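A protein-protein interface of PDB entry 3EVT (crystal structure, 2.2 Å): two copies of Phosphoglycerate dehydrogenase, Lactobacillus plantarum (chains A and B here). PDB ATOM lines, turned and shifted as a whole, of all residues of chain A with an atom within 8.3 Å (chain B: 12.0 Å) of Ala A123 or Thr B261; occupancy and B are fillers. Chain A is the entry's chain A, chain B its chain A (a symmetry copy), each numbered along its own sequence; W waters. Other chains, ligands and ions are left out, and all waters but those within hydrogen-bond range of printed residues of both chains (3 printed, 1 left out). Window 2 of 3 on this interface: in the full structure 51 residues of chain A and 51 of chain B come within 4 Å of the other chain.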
ATOM      1  N   ALA A 116     -15.429   7.367  19.241  1.00  0.00           N
ATOM      2  CA  ALA A 116     -16.591   7.963  18.545  1.00  0.00           C
ATOM      3  C   ALA A 116     -17.410   8.866  19.436  1.00  0.00           C
ATOM      4  O   ALA A 116     -17.871   9.906  18.988  1.00  0.00           O
ATOM      5  CB  ALA A 116     -17.475   6.931  17.924  1.00  0.00           C
ATOM      6  N   TRP A 117     -17.589   8.479  20.687  1.00  0.00           N
ATOM      7  CA  TRP A 117     -18.298   9.326  21.644  1.00  0.00           C
ATOM      8  C   TRP A 117     -17.571  10.627  21.953  1.00  0.00           C
ATOM      9  O   TRP A 117     -18.191  11.682  21.954  1.00  0.00           O
ATOM     10  CB  TRP A 117     -18.671   8.587  22.946  1.00  0.00           C
ATOM     11  CG  TRP A 117     -19.650   9.423  23.691  1.00  0.00           C
ATOM     12  CD1 TRP A 117     -19.399  10.196  24.792  1.00  0.00           C
ATOM     13  CD2 TRP A 117     -21.024   9.690  23.312  1.00  0.00           C
ATOM     14  NE1 TRP A 117     -20.535  10.886  25.135  1.00  0.00           N
ATOM     15  CE2 TRP A 117     -21.539  10.597  24.252  1.00  0.00           C
ATOM     16  CE3 TRP A 117     -21.864   9.236  22.270  1.00  0.00           C
ATOM     17  CZ2 TRP A 117     -22.867  11.050  24.206  1.00  0.00           C
ATOM     18  CZ3 TRP A 117     -23.177   9.685  22.219  1.00  0.00           C
ATOM     19  CH2 TRP A 117     -23.670  10.585  23.174  1.00  0.00           C
ATOM     20  N   LEU A 118     -16.266  10.570  22.164  1.00  0.00           N
ATOM     21  CA  LEU A 118     -15.489  11.790  22.363  1.00  0.00           C
ATOM     22  C   LEU A 118     -15.595  12.695  21.136  1.00  0.00           C
ATOM     23  O   LEU A 118     -15.673  13.918  21.257  1.00  0.00           O
ATOM     24  CB  LEU A 118     -14.031  11.440  22.637  1.00  0.00           C
ATOM     25  CG  LEU A 118     -13.733  10.580  23.870  1.00  0.00           C
ATOM     26  CD1 LEU A 118     -12.206  10.348  23.905  1.00  0.00           C
ATOM     27  CD2 LEU A 118     -14.196  11.251  25.174  1.00  0.00           C
ATOM     28  N   ASN A 119     -15.620  12.078  19.945  1.00  0.00           N
ATOM     29  CA  ASN A 119     -15.831  12.796  18.702  1.00  0.00           C
ATOM     30  C   ASN A 119     -17.207  13.433  18.649  1.00  0.00           C
ATOM     31  O   ASN A 119     -17.338  14.621  18.289  1.00  0.00           O
ATOM     32  CB  ASN A 119     -15.627  11.895  17.484  1.00  0.00           C
ATOM     33  CG  ASN A 119     -15.902  12.639  16.157  1.00  0.00           C
ATOM     34  OD1 ASN A 119     -15.254  13.658  15.861  1.00  0.00           O
ATOM     35  ND2 ASN A 119     -16.906  12.178  15.389  1.00  0.00           N
ATOM     36  N   GLN A 120     -18.235  12.667  19.013  1.00  0.00           N
ATOM     37  CA  GLN A 120     -19.629  13.165  19.055  1.00  0.00           C
ATOM     38  C   GLN A 120     -19.846  14.323  20.085  1.00  0.00           C
ATOM     39  O   GLN A 120     -20.718  15.228  19.874  1.00  0.00           O
ATOM     40  CB  GLN A 120     -20.590  11.987  19.312  1.00  0.00           C
ATOM     41  CG  GLN A 120     -22.062  12.317  19.679  1.00  0.00           C
ATOM     42  CD  GLN A 120     -23.019  11.171  19.322  1.00  0.00           C
ATOM     43  OE1 GLN A 120     -22.569  10.091  18.958  1.00  0.00           O
ATOM     44  NE2 GLN A 120     -24.335  11.386  19.469  1.00  0.00           N
ATOM     45  N   ARG A 121     -19.104  14.283  21.201  1.00  0.00           N
ATOM     46  CA  ARG A 121     -19.165  15.368  22.165  1.00  0.00           C
ATOM     47  C   ARG A 121     -18.079  16.397  21.868  1.00  0.00           C
ATOM     48  O   ARG A 121     -17.808  17.273  22.692  1.00  0.00           O
ATOM     49  CB  ARG A 121     -19.032  14.840  23.594  1.00  0.00           C
ATOM     50  CG  ARG A 121     -20.343  14.235  24.055  1.00  0.00           C
ATOM     51  CD  ARG A 121     -21.402  15.332  24.227  1.00  0.00           C
ATOM     52  NE  ARG A 121     -22.763  14.792  24.326  1.00  0.00           N
ATOM     53  CZ  ARG A 121     -23.567  14.593  23.284  1.00  0.00           C
ATOM     54  NH1 ARG A 121     -23.143  14.872  22.046  1.00  0.00           N
ATOM     55  NH2 ARG A 121     -24.793  14.098  23.473  1.00  0.00           N
ATOM     56  N   GLY A 122     -17.451  16.278  20.700  1.00  0.00           N
ATOM     57  CA  GLY A 122     -16.283  17.117  20.387  1.00  0.00           C
ATOM     58  C   GLY A 122     -16.441  17.737  19.028  1.00  0.00           C
ATOM     59  O   GLY A 122     -17.466  18.337  18.731  1.00  0.00           O
ATOM     60  N   ALA A 123     -15.443  17.567  18.194  1.00  0.00           N
ATOM     61  CA  ALA A 123     -15.472  18.139  16.858  1.00  0.00           C
ATOM     62  C   ALA A 123     -16.520  17.549  15.886  1.00  0.00           C
ATOM     63  O   ALA A 123     -16.858  18.179  14.878  1.00  0.00           O
ATOM     64  CB  ALA A 123     -14.034  18.101  16.232  1.00  0.00           C
ATOM     65  N   ARG A 124     -17.030  16.347  16.165  1.00  0.00           N
ATOM     66  CA  ARG A 124     -17.984  15.699  15.243  1.00  0.00           C
ATOM     67  C   ARG A 124     -17.443  15.641  13.839  1.00  0.00           C
ATOM     68  O   ARG A 124     -18.123  15.980  12.861  1.00  0.00           O
ATOM     69  CB  ARG A 124     -19.334  16.416  15.238  1.00  0.00           C
ATOM     70  CG  ARG A 124     -19.955  16.520  16.619  1.00  0.00           C
ATOM     71  CD  ARG A 124     -21.019  17.591  16.656  1.00  0.00           C
ATOM     72  NE  ARG A 124     -21.671  17.632  17.957  1.00  0.00           N
ATOM     73  CZ  ARG A 124     -22.815  18.267  18.207  1.00  0.00           C
ATOM     74  NH1 ARG A 124     -23.485  18.890  17.226  1.00  0.00           N
ATOM     75  NH2 ARG A 124     -23.313  18.238  19.435  1.00  0.00           N
ATOM     76  N   GLN A 125     -16.208  15.192  13.730  1.00  0.00           N
ATOM     77  CA  GLN A 125     -15.641  14.913  12.437  1.00  0.00           C
ATOM     78  C   GLN A 125     -16.191  13.599  11.885  1.00  0.00           C
ATOM     79  O   GLN A 125     -16.824  12.838  12.620  1.00  0.00           O
ATOM     80  CB  GLN A 125     -14.094  14.944  12.514  1.00  0.00           C
ATOM     81  CG  GLN A 125     -13.553  16.402  12.797  1.00  0.00           C
ATOM     82  CD  GLN A 125     -14.169  17.424  11.793  1.00  0.00           C
ATOM     83  OE1 GLN A 125     -13.835  17.379  10.608  1.00  0.00           O
ATOM     84  NE2 GLN A 125     -15.115  18.295  12.258  1.00  0.00           N
ATOM     85  N   TRP A 126     -15.979  13.361  10.589  1.00  0.00           N
ATOM     86  CA  TRP A 126     -16.399  12.127   9.987  1.00  0.00           C
ATOM     87  C   TRP A 126     -15.193  11.211   9.897  1.00  0.00           C
ATOM     88  O   TRP A 126     -14.967  10.574   8.906  1.00  0.00           O
ATOM     89  CB  TRP A 126     -17.060  12.311   8.623  1.00  0.00           C
ATOM     90  CG  TRP A 126     -17.993  11.154   8.275  1.00  0.00           C
ATOM     91  CD1 TRP A 126     -17.840  10.233   7.262  1.00  0.00           C
ATOM     92  CD2 TRP A 126     -19.203  10.776   8.978  1.00  0.00           C
ATOM     93  NE1 TRP A 126     -18.871   9.329   7.305  1.00  0.00           N
ATOM     94  CE2 TRP A 126     -19.717   9.637   8.336  1.00  0.00           C
ATOM     95  CE3 TRP A 126     -19.879  11.286  10.090  1.00  0.00           C
ATOM     96  CZ2 TRP A 126     -20.893   9.004   8.757  1.00  0.00           C
ATOM     97  CZ3 TRP A 126     -21.041  10.660  10.512  1.00  0.00           C
ATOM     98  CH2 TRP A 126     -21.546   9.539   9.835  1.00  0.00           C
ATOM     99  N   ALA A 127     -14.447  11.119  10.978  1.00  0.00           N
ATOM    100  CA  ALA A 127     -13.346  10.203  11.057  1.00  0.00           C
ATOM    101  C   ALA A 127     -12.889  10.243  12.501  1.00  0.00           C
ATOM    102  O   ALA A 127     -13.211  11.162  13.245  1.00  0.00           O
ATOM    103  CB  ALA A 127     -12.219  10.641  10.099  1.00  0.00           C
ATOM    104  N   MET B 238     -35.882   9.782  15.622  1.00  0.00           N
ATOM    105  CA  MET B 238     -35.847  10.684  16.757  1.00  0.00           C
ATOM    106  C   MET B 238     -37.174  10.720  17.510  1.00  0.00           C
ATOM    107  O   MET B 238     -37.173  10.746  18.750  1.00  0.00           O
ATOM    108  CB  MET B 238     -35.352  12.077  16.356  1.00  0.00           C
ATOM    109  CG  MET B 238     -33.826  12.085  16.022  1.00  0.00           C
ATOM    110  SD  MET B 238     -33.178  13.747  15.778  1.00  0.00           S
ATOM    111  CE  MET B 238     -33.896  13.982  14.160  1.00  0.00           C
ATOM    112  N   THR B 254     -25.430   7.271   7.977  1.00  0.00           N
ATOM    113  CA  THR B 254     -26.449   8.292   8.191  1.00  0.00           C
ATOM    114  C   THR B 254     -26.972   8.826   6.843  1.00  0.00           C
ATOM    115  O   THR B 254     -26.358   8.587   5.786  1.00  0.00           O
ATOM    116  CB  THR B 254     -25.934   9.417   9.129  1.00  0.00           C
ATOM    117  OG1 THR B 254     -24.797  10.101   8.541  1.00  0.00           O
ATOM    118  CG2 THR B 254     -25.498   8.783  10.433  1.00  0.00           C
ATOM    119  N   GLU B 255     -28.152   9.457   6.889  1.00  0.00           N
ATOM    120  CA  GLU B 255     -28.691  10.265   5.777  1.00  0.00           C
ATOM    121  C   GLU B 255     -29.001  11.670   6.281  1.00  0.00           C
ATOM    122  O   GLU B 255     -29.977  11.856   7.008  1.00  0.00           O
ATOM    123  CB  GLU B 255     -29.984   9.675   5.300  1.00  0.00           C
ATOM    124  CG  GLU B 255     -30.741  10.568   4.395  1.00  0.00           C
ATOM    125  CD  GLU B 255     -31.990   9.881   3.875  1.00  0.00           C
ATOM    126  OE1 GLU B 255     -32.884   9.546   4.682  1.00  0.00           O
ATOM    127  OE2 GLU B 255     -32.065   9.651   2.650  1.00  0.00           O
ATOM    128  N   PRO B 256     -28.185  12.674   5.898  1.00  0.00           N
ATOM    129  CA  PRO B 256     -27.082  12.601   4.933  1.00  0.00           C
ATOM    130  C   PRO B 256     -25.802  12.085   5.560  1.00  0.00           C
ATOM    131  O   PRO B 256     -25.715  11.953   6.769  1.00  0.00           O
ATOM    132  CB  PRO B 256     -26.885  14.074   4.529  1.00  0.00           C
ATOM    133  CG  PRO B 256     -27.238  14.848   5.787  1.00  0.00           C
ATOM    134  CD  PRO B 256     -28.346  14.033   6.464  1.00  0.00           C
ATOM    135  N   GLU B 257     -24.806  11.823   4.730  1.00  0.00           N
ATOM    136  CA  GLU B 257     -23.496  11.409   5.202  1.00  0.00           C
ATOM    137  C   GLU B 257     -22.443  12.083   4.338  1.00  0.00           C
ATOM    138  O   GLU B 257     -22.527  12.001   3.127  1.00  0.00           O
ATOM    139  CB  GLU B 257     -23.367   9.876   5.051  1.00  0.00           C
ATOM    140  CG  GLU B 257     -22.230   9.203   5.835  1.00  0.00           C
ATOM    141  CD  GLU B 257     -22.262   7.692   5.627  1.00  0.00           C
ATOM    142  OE1 GLU B 257     -23.331   7.116   5.819  1.00  0.00           O
ATOM    143  OE2 GLU B 257     -21.256   7.089   5.219  1.00  0.00           O
ATOM    144  N   PRO B 258     -21.437  12.724   4.946  1.00  0.00           N
ATOM    145  CA  PRO B 258     -21.245  12.868   6.391  1.00  0.00           C
ATOM    146  C   PRO B 258     -22.436  13.466   7.066  1.00  0.00           C
ATOM    147  O   PRO B 258     -23.163  14.252   6.449  1.00  0.00           O
ATOM    148  CB  PRO B 258     -20.087  13.859   6.508  1.00  0.00           C
ATOM    149  CG  PRO B 258     -19.286  13.627   5.279  1.00  0.00           C
ATOM    150  CD  PRO B 258     -20.261  13.170   4.183  1.00  0.00           C
ATOM    151  N   LEU B 259     -22.626  13.125   8.338  1.00  0.00           N
ATOM    152  CA  LEU B 259     -23.598  13.846   9.146  1.00  0.00           C
ATOM    153  C   LEU B 259     -23.020  15.209   9.475  1.00  0.00           C
ATOM    154  O   LEU B 259     -22.009  15.293  10.195  1.00  0.00           O
ATOM    155  CB  LEU B 259     -23.922  13.111  10.441  1.00  0.00           C
ATOM    156  CG  LEU B 259     -25.253  13.535  11.063  1.00  0.00           C
ATOM    157  CD1 LEU B 259     -26.399  13.102  10.135  1.00  0.00           C
ATOM    158  CD2 LEU B 259     -25.388  12.943  12.497  1.00  0.00           C
ATOM    159  N   PRO B 260     -23.651  16.289   8.963  1.00  0.00           N
ATOM    160  CA  PRO B 260     -23.215  17.684   9.251  1.00  0.00           C
ATOM    161  C   PRO B 260     -23.172  17.985  10.744  1.00  0.00           C
ATOM    162  O   PRO B 260     -24.055  17.530  11.493  1.00  0.00           O
ATOM    163  CB  PRO B 260     -24.305  18.535   8.610  1.00  0.00           C
ATOM    164  CG  PRO B 260     -24.959  17.614   7.551  1.00  0.00           C
ATOM    165  CD  PRO B 260     -24.882  16.240   8.144  1.00  0.00           C
ATOM    166  N   THR B 261     -22.209  18.811  11.155  1.00  0.00           N
ATOM    167  CA  THR B 261     -21.891  18.993  12.558  1.00  0.00           C
ATOM    168  C   THR B 261     -22.977  19.656  13.381  1.00  0.00           C
ATOM    169  O   THR B 261     -22.914  19.663  14.602  1.00  0.00           O
ATOM    170  CB  THR B 261     -20.595  19.806  12.749  1.00  0.00           C
ATOM    171  OG1 THR B 261     -20.759  21.116  12.176  1.00  0.00           O
ATOM    172  CG2 THR B 261     -19.384  19.086  12.134  1.00  0.00           C
ATOM    173  N   ASP B 262     -23.975  20.222  12.709  1.00  0.00           N
ATOM    174  CA  ASP B 262     -25.062  20.883  13.399  1.00  0.00           C
ATOM    175  C   ASP B 262     -26.308  20.013  13.360  1.00  0.00           C
ATOM    176  O   ASP B 262     -27.376  20.463  13.758  1.00  0.00           O
ATOM    177  CB  ASP B 262     -25.364  22.209  12.705  1.00  0.00           C
ATOM    178  CG  ASP B 262     -25.414  22.069  11.172  1.00  0.00           C
ATOM    179  OD1 ASP B 262     -25.808  21.005  10.622  1.00  0.00           O
ATOM    180  OD2 ASP B 262     -25.041  23.036  10.492  1.00  0.00           O
ATOM    181  N   HIS B 263     -26.201  18.794  12.841  1.00  0.00           N
ATOM    182  CA  HIS B 263     -27.346  17.887  12.851  1.00  0.00           C
ATOM    183  C   HIS B 263     -27.768  17.542  14.292  1.00  0.00           C
ATOM    184  O   HIS B 263     -26.905  17.362  15.172  1.00  0.00           O
ATOM    185  CB  HIS B 263     -27.051  16.617  12.059  1.00  0.00           C
ATOM    186  CG  HIS B 263     -28.281  15.915  11.602  1.00  0.00           C
ATOM    187  ND1 HIS B 263     -29.081  15.192  12.460  1.00  0.00           N
ATOM    188  CD2 HIS B 263     -28.876  15.856  10.384  1.00  0.00           C
ATOM    189  CE1 HIS B 263     -30.109  14.707  11.789  1.00  0.00           C
ATOM    190  NE2 HIS B 263     -30.005  15.090  10.525  1.00  0.00           N
ATOM    191  N   PRO B 264     -29.089  17.481  14.539  1.00  0.00           N
ATOM    192  CA  PRO B 264     -29.533  17.293  15.936  1.00  0.00           C
ATOM    193  C   PRO B 264     -29.298  15.869  16.475  1.00  0.00           C
ATOM    194  O   PRO B 264     -29.202  15.683  17.700  1.00  0.00           O
ATOM    195  CB  PRO B 264     -31.025  17.714  15.928  1.00  0.00           C
ATOM    196  CG  PRO B 264     -31.433  17.850  14.458  1.00  0.00           C
ATOM    197  CD  PRO B 264     -30.191  17.825  13.609  1.00  0.00           C
ATOM    198  N   LEU B 265     -29.158  14.891  15.577  1.00  0.00           N
ATOM    199  CA  LEU B 265     -28.728  13.522  15.973  1.00  0.00           C
ATOM    200  C   LEU B 265     -27.487  13.509  16.858  1.00  0.00           C
ATOM    201  O   LEU B 265     -27.389  12.717  17.808  1.00  0.00           O
ATOM    202  CB  LEU B 265     -28.469  12.609  14.751  1.00  0.00           C
ATOM    203  CG  LEU B 265     -29.641  11.888  14.103  1.00  0.00           C
ATOM    204  CD1 LEU B 265     -29.131  11.023  12.995  1.00  0.00           C
ATOM    205  CD2 LEU B 265     -30.477  11.051  15.136  1.00  0.00           C
ATOM    206  N   TRP B 266     -26.525  14.364  16.545  1.00  0.00           N
ATOM    207  CA  TRP B 266     -25.297  14.413  17.370  1.00  0.00           C
ATOM    208  C   TRP B 266     -25.524  14.793  18.833  1.00  0.00           C
ATOM    209  O   TRP B 266     -24.779  14.346  19.705  1.00  0.00           O
ATOM    210  CB  TRP B 266     -24.292  15.426  16.845  1.00  0.00           C
ATOM    211  CG  TRP B 266     -23.616  15.151  15.494  1.00  0.00           C
ATOM    212  CD1 TRP B 266     -23.901  15.762  14.299  1.00  0.00           C
ATOM    213  CD2 TRP B 266     -22.486  14.280  15.239  1.00  0.00           C
ATOM    214  NE1 TRP B 266     -23.025  15.315  13.329  1.00  0.00           N
ATOM    215  CE2 TRP B 266     -22.153  14.413  13.879  1.00  0.00           C
ATOM    216  CE3 TRP B 266     -21.725  13.419  16.038  1.00  0.00           C
ATOM    217  CZ2 TRP B 266     -21.096  13.706  13.288  1.00  0.00           C
ATOM    218  CZ3 TRP B 266     -20.674  12.711  15.457  1.00  0.00           C
ATOM    219  CH2 TRP B 266     -20.387  12.842  14.078  1.00  0.00           C
ATOM    220  N   GLN B 267     -26.487  15.685  19.080  1.00  0.00           N
ATOM    221  CA  GLN B 267     -26.720  16.192  20.432  1.00  0.00           C
ATOM    222  C   GLN B 267     -27.476  15.229  21.319  1.00  0.00           C
ATOM    223  O   GLN B 267     -27.595  15.506  22.496  1.00  0.00           O
ATOM    224  CB  GLN B 267     -27.523  17.517  20.430  1.00  0.00           C
ATOM    225  CG  GLN B 267     -27.669  18.180  19.079  1.00  0.00           C
ATOM    226  CD  GLN B 267     -26.457  19.053  18.724  1.00  0.00           C
ATOM    227  OE1 GLN B 267     -25.676  19.436  19.622  1.00  0.00           O
ATOM    228  NE2 GLN B 267     -26.281  19.354  17.409  1.00  0.00           N
ATOM    229  N   ARG B 268     -28.000  14.117  20.784  1.00  0.00           N
ATOM    230  CA  ARG B 268     -28.699  13.134  21.632  1.00  0.00           C
ATOM    231  C   ARG B 268     -27.705  12.276  22.463  1.00  0.00           C
ATOM    232  O   ARG B 268     -26.593  11.959  21.992  1.00  0.00           O
ATOM    233  CB  ARG B 268     -29.581  12.237  20.786  1.00  0.00           C
ATOM    234  CG  ARG B 268     -30.228  12.925  19.538  1.00  0.00           C
ATOM    235  CD  ARG B 268     -31.756  12.996  19.579  1.00  0.00           C
ATOM    236  NE  ARG B 268     -32.440  11.964  20.375  1.00  0.00           N
ATOM    237  CZ  ARG B 268     -33.762  11.965  20.624  1.00  0.00           C
ATOM    238  NH1 ARG B 268     -34.322  11.012  21.368  1.00  0.00           N
ATOM    239  NH2 ARG B 268     -34.541  12.915  20.112  1.00  0.00           N
ATOM    240  N   ILE B 273     -23.218   7.855  17.265  1.00  0.00           N
ATOM    241  CA  ILE B 273     -22.855   8.044  15.875  1.00  0.00           C
ATOM    242  C   ILE B 273     -21.424   7.569  15.718  1.00  0.00           C
ATOM    243  O   ILE B 273     -20.532   8.024  16.455  1.00  0.00           O
ATOM    244  CB  ILE B 273     -22.914   9.587  15.463  1.00  0.00           C
ATOM    245  CG1 ILE B 273     -24.252  10.194  15.831  1.00  0.00           C
ATOM    246  CG2 ILE B 273     -22.662   9.769  13.947  1.00  0.00           C
ATOM    247  CD1 ILE B 273     -25.428   9.627  15.006  1.00  0.00           C
ATOM    248  N   THR B 274     -21.178   6.657  14.791  1.00  0.00           N
ATOM    249  CA  THR B 274     -19.813   6.375  14.461  1.00  0.00           C
ATOM    250  C   THR B 274     -19.700   6.679  12.986  1.00  0.00           C
ATOM    251  O   THR B 274     -20.614   6.402  12.237  1.00  0.00           O
ATOM    252  CB  THR B 274     -19.386   4.891  14.756  1.00  0.00           C
ATOM    253  OG1 THR B 274     -20.256   3.998  14.037  1.00  0.00           O
ATOM    254  CG2 THR B 274     -19.487   4.608  16.248  1.00  0.00           C
ATOM    255  N   PRO B 275     -18.558   7.261  12.572  1.00  0.00           N
ATOM    256  CA  PRO B 275     -18.442   7.747  11.199  1.00  0.00           C
ATOM    257  C   PRO B 275     -18.106   6.693  10.181  1.00  0.00           C
ATOM    258  O   PRO B 275     -17.018   6.740   9.635  1.00  0.00           O
ATOM    259  CB  PRO B 275     -17.305   8.764  11.287  1.00  0.00           C
ATOM    260  CG  PRO B 275     -16.442   8.301  12.388  1.00  0.00           C
ATOM    261  CD  PRO B 275     -17.338   7.523  13.374  1.00  0.00           C
HETATM  262  O   HOH W   1     -18.919   8.195   4.505  1.00  0.00           O
HETATM  263  O   HOH W   2     -19.370  15.215  10.520  1.00  0.00           O
HETATM  264  O   HOH W   3     -18.490  10.048  16.342  1.00  0.00           O
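Among the printed residues, merely in contact across the chains: Ala A116 with Ile B273 (3.6 Å), Ala A116 with Thr B274 (3.5 Å), Trp A117 with Arg B268 (3.4 Å), Asn A119 with Trp B266 (3.8 Å), Gln A120 with Leu B265 (3.7 Å), Ala A123 with Thr B261 (3.8 Å), Arg A124 with Trp B266 (3.5 Å), Gln A125 with Trp B266 (3.8 Å), Trp A126 with Thr B254 (3.5 Å), Trp A126 with Glu B257 (3.2 Å), Trp A126 with Pro B258 (3.9 Å), Trp A126 with Leu B259 (3.6 Å), Trp A126 with Ile B273 (3.9 Å), Trp A126 with Pro B275 (3.5 Å) and Ala A127 with Pro B275 (3.7 Å).
Water W2 lies within hydrogen-bond range of O of Leu B259 (2.7 Å) and O of Arg A124 (2.8 Å).
Water W1 lies within hydrogen-bond range of OE2 of Glu B257 and NE1 of Trp A126.
Water W3 lies within hydrogen-bond range of O of Ala A116, ND2 of Asn A119 and O of Ile B273.
No position is printed for both chains.
Of the 23 pairs that touch across the chains among the printed residues, none has its exchanged pair printed and touching as well.
OE1 of Glu B257 is in hydrogen-bond range of N of Thr B254 (3.0 Å).
The side-chain hydroxyl (OG1) of Thr B254 is in hydrogen-bond range of the backbone carbonyl oxygen (O) of Pro B256.
The backbone carbonyl oxygen of Ala A123 lies within hydrogen-bond range of the side-chain amide nitrogen of Gln A125, at 3.1 Å.
The backbone carbonyl oxygen of Pro B260 sits at hydrogen-bond distance from the indole nitrogen of Trp B266 (3.1 Å).
The backbone carbonyl oxygen (O) of His B263 sits at hydrogen-bond distance from the side-chain amide nitrogen (NE2) of Gln B267, at 3.1 Å.
OD1 of Asn A119 sits at hydrogen-bond distance from N of Gln A125 (2.8 Å).
Of the 19 printed residues of chain B, 12 touch a printed residue of chain A.
Printed residues of chain B that touch a printed residue of chain A: Thr B254, Glu B257, Pro B258, Leu B259, Thr B261, Leu B265, Trp B266, Gln B267, Arg B268, Ile B273, Thr B274 and Pro B275.
Hydrophobic or aromatic side chains of chain B within 4 Å of the printed part of chain A: Pro B258, Leu B259, Trp B266, Ile B273 and Pro B275.
Of the 12 printed residues of chain A, 10 touch a printed residue of chain B.
Printed residues of chain A that touch a printed residue of chain B: Ala A116, Trp A117, Asn A119, Gln A120, Arg A121, Ala A123, Arg A124, Gln A125, Trp A126 and Ala A127.
Hydrophobic or aromatic side chains of chain A that line the printed part of chain B: Ala A116, Trp A117 and Trp A126.
Along chain A the printed residues that touch a printed residue of chain B span positions 116 to 127.
Among the printed residues, 23 pairs touch across the chains.
Among the printed residues, no Asp or Glu carboxylate lies within 4 Å of a Lys or Arg side-chain nitrogen of the other chain.
The backbone carbonyl oxygen (O) of Trp B266 is in hydrogen-bond range of the side-chain amide nitrogen (NE2) of Gln A120.
NH1 of Arg A121 is in hydrogen-bond range of O of Trp B266 (2.9 Å).
O of Gln B267 lies within hydrogen-bond range of NH2 of Arg A121, at 3.3 Å.
The side-chain amide oxygen (OE1) of Gln A120 is in hydrogen-bond range of the backbone NH (N) of Ile B273 (2.9 Å).
O of Arg B268 sits at hydrogen-bond distance from NE2 of Gln A120, 3.4 Å away.
NH2 of Arg A124 lies within hydrogen-bond range of OE1 of Gln B267 (2.7 Å).
The guanidinium group (NH2) of Arg A121 lies within hydrogen-bond range of the backbone carbonyl oxygen (O) of Arg B268 (3.2 Å).
The backbone carbonyl oxygen (O) of Thr B261 sits at hydrogen-bond distance from the guanidinium group (NH1) of Arg A124 (2.8 Å).
Of chain B, only Thr B261 comes within 4 Å of Ala A123.
Asn A119 touches one residue of chain B.
Arg A124 touches just these residues of chain B: Thr B261, Trp B266 and Gln B267.
Gln A125 touches just one residue of chain B: Trp B266.
Of the printed residues of chain A, Thr B274 touches Ala A116 (3.5 Å).
Of the printed residues of chain A, Trp B266 touches Asn A119 (3.8 Å), Gln A120 (3.0 Å), Arg A121 (2.9 Å), Arg A124 (3.5 Å) and Gln A125 (3.8 Å).
Printed residues of chain B within 4 Å of Gln A120: Leu B265 (3.7 Å), Trp B266 (3.0 Å), Arg B268 (3.4 Å) and Ile B273 (2.9 Å).
Of the printed residues of chain B, Ala A127 touches Pro B275 (3.7 Å).
Printed residues of chain B within 4 Å of Trp A126: Thr B254, Glu B257, Pro B258, Leu B259, Ile B273 and Pro B275.
Pro B260 touches none of the printed residues of chain A.
The nearest residue of chain B that does not touch Ala A123 is Trp B266 (6.4 Å).
The nearest residue of chain A that does not touch Thr B261 is Gln A125 (4.3 Å).
The nearest printed residue of chain A that does not touch Pro B258 is Gln A125 (6.6 Å).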
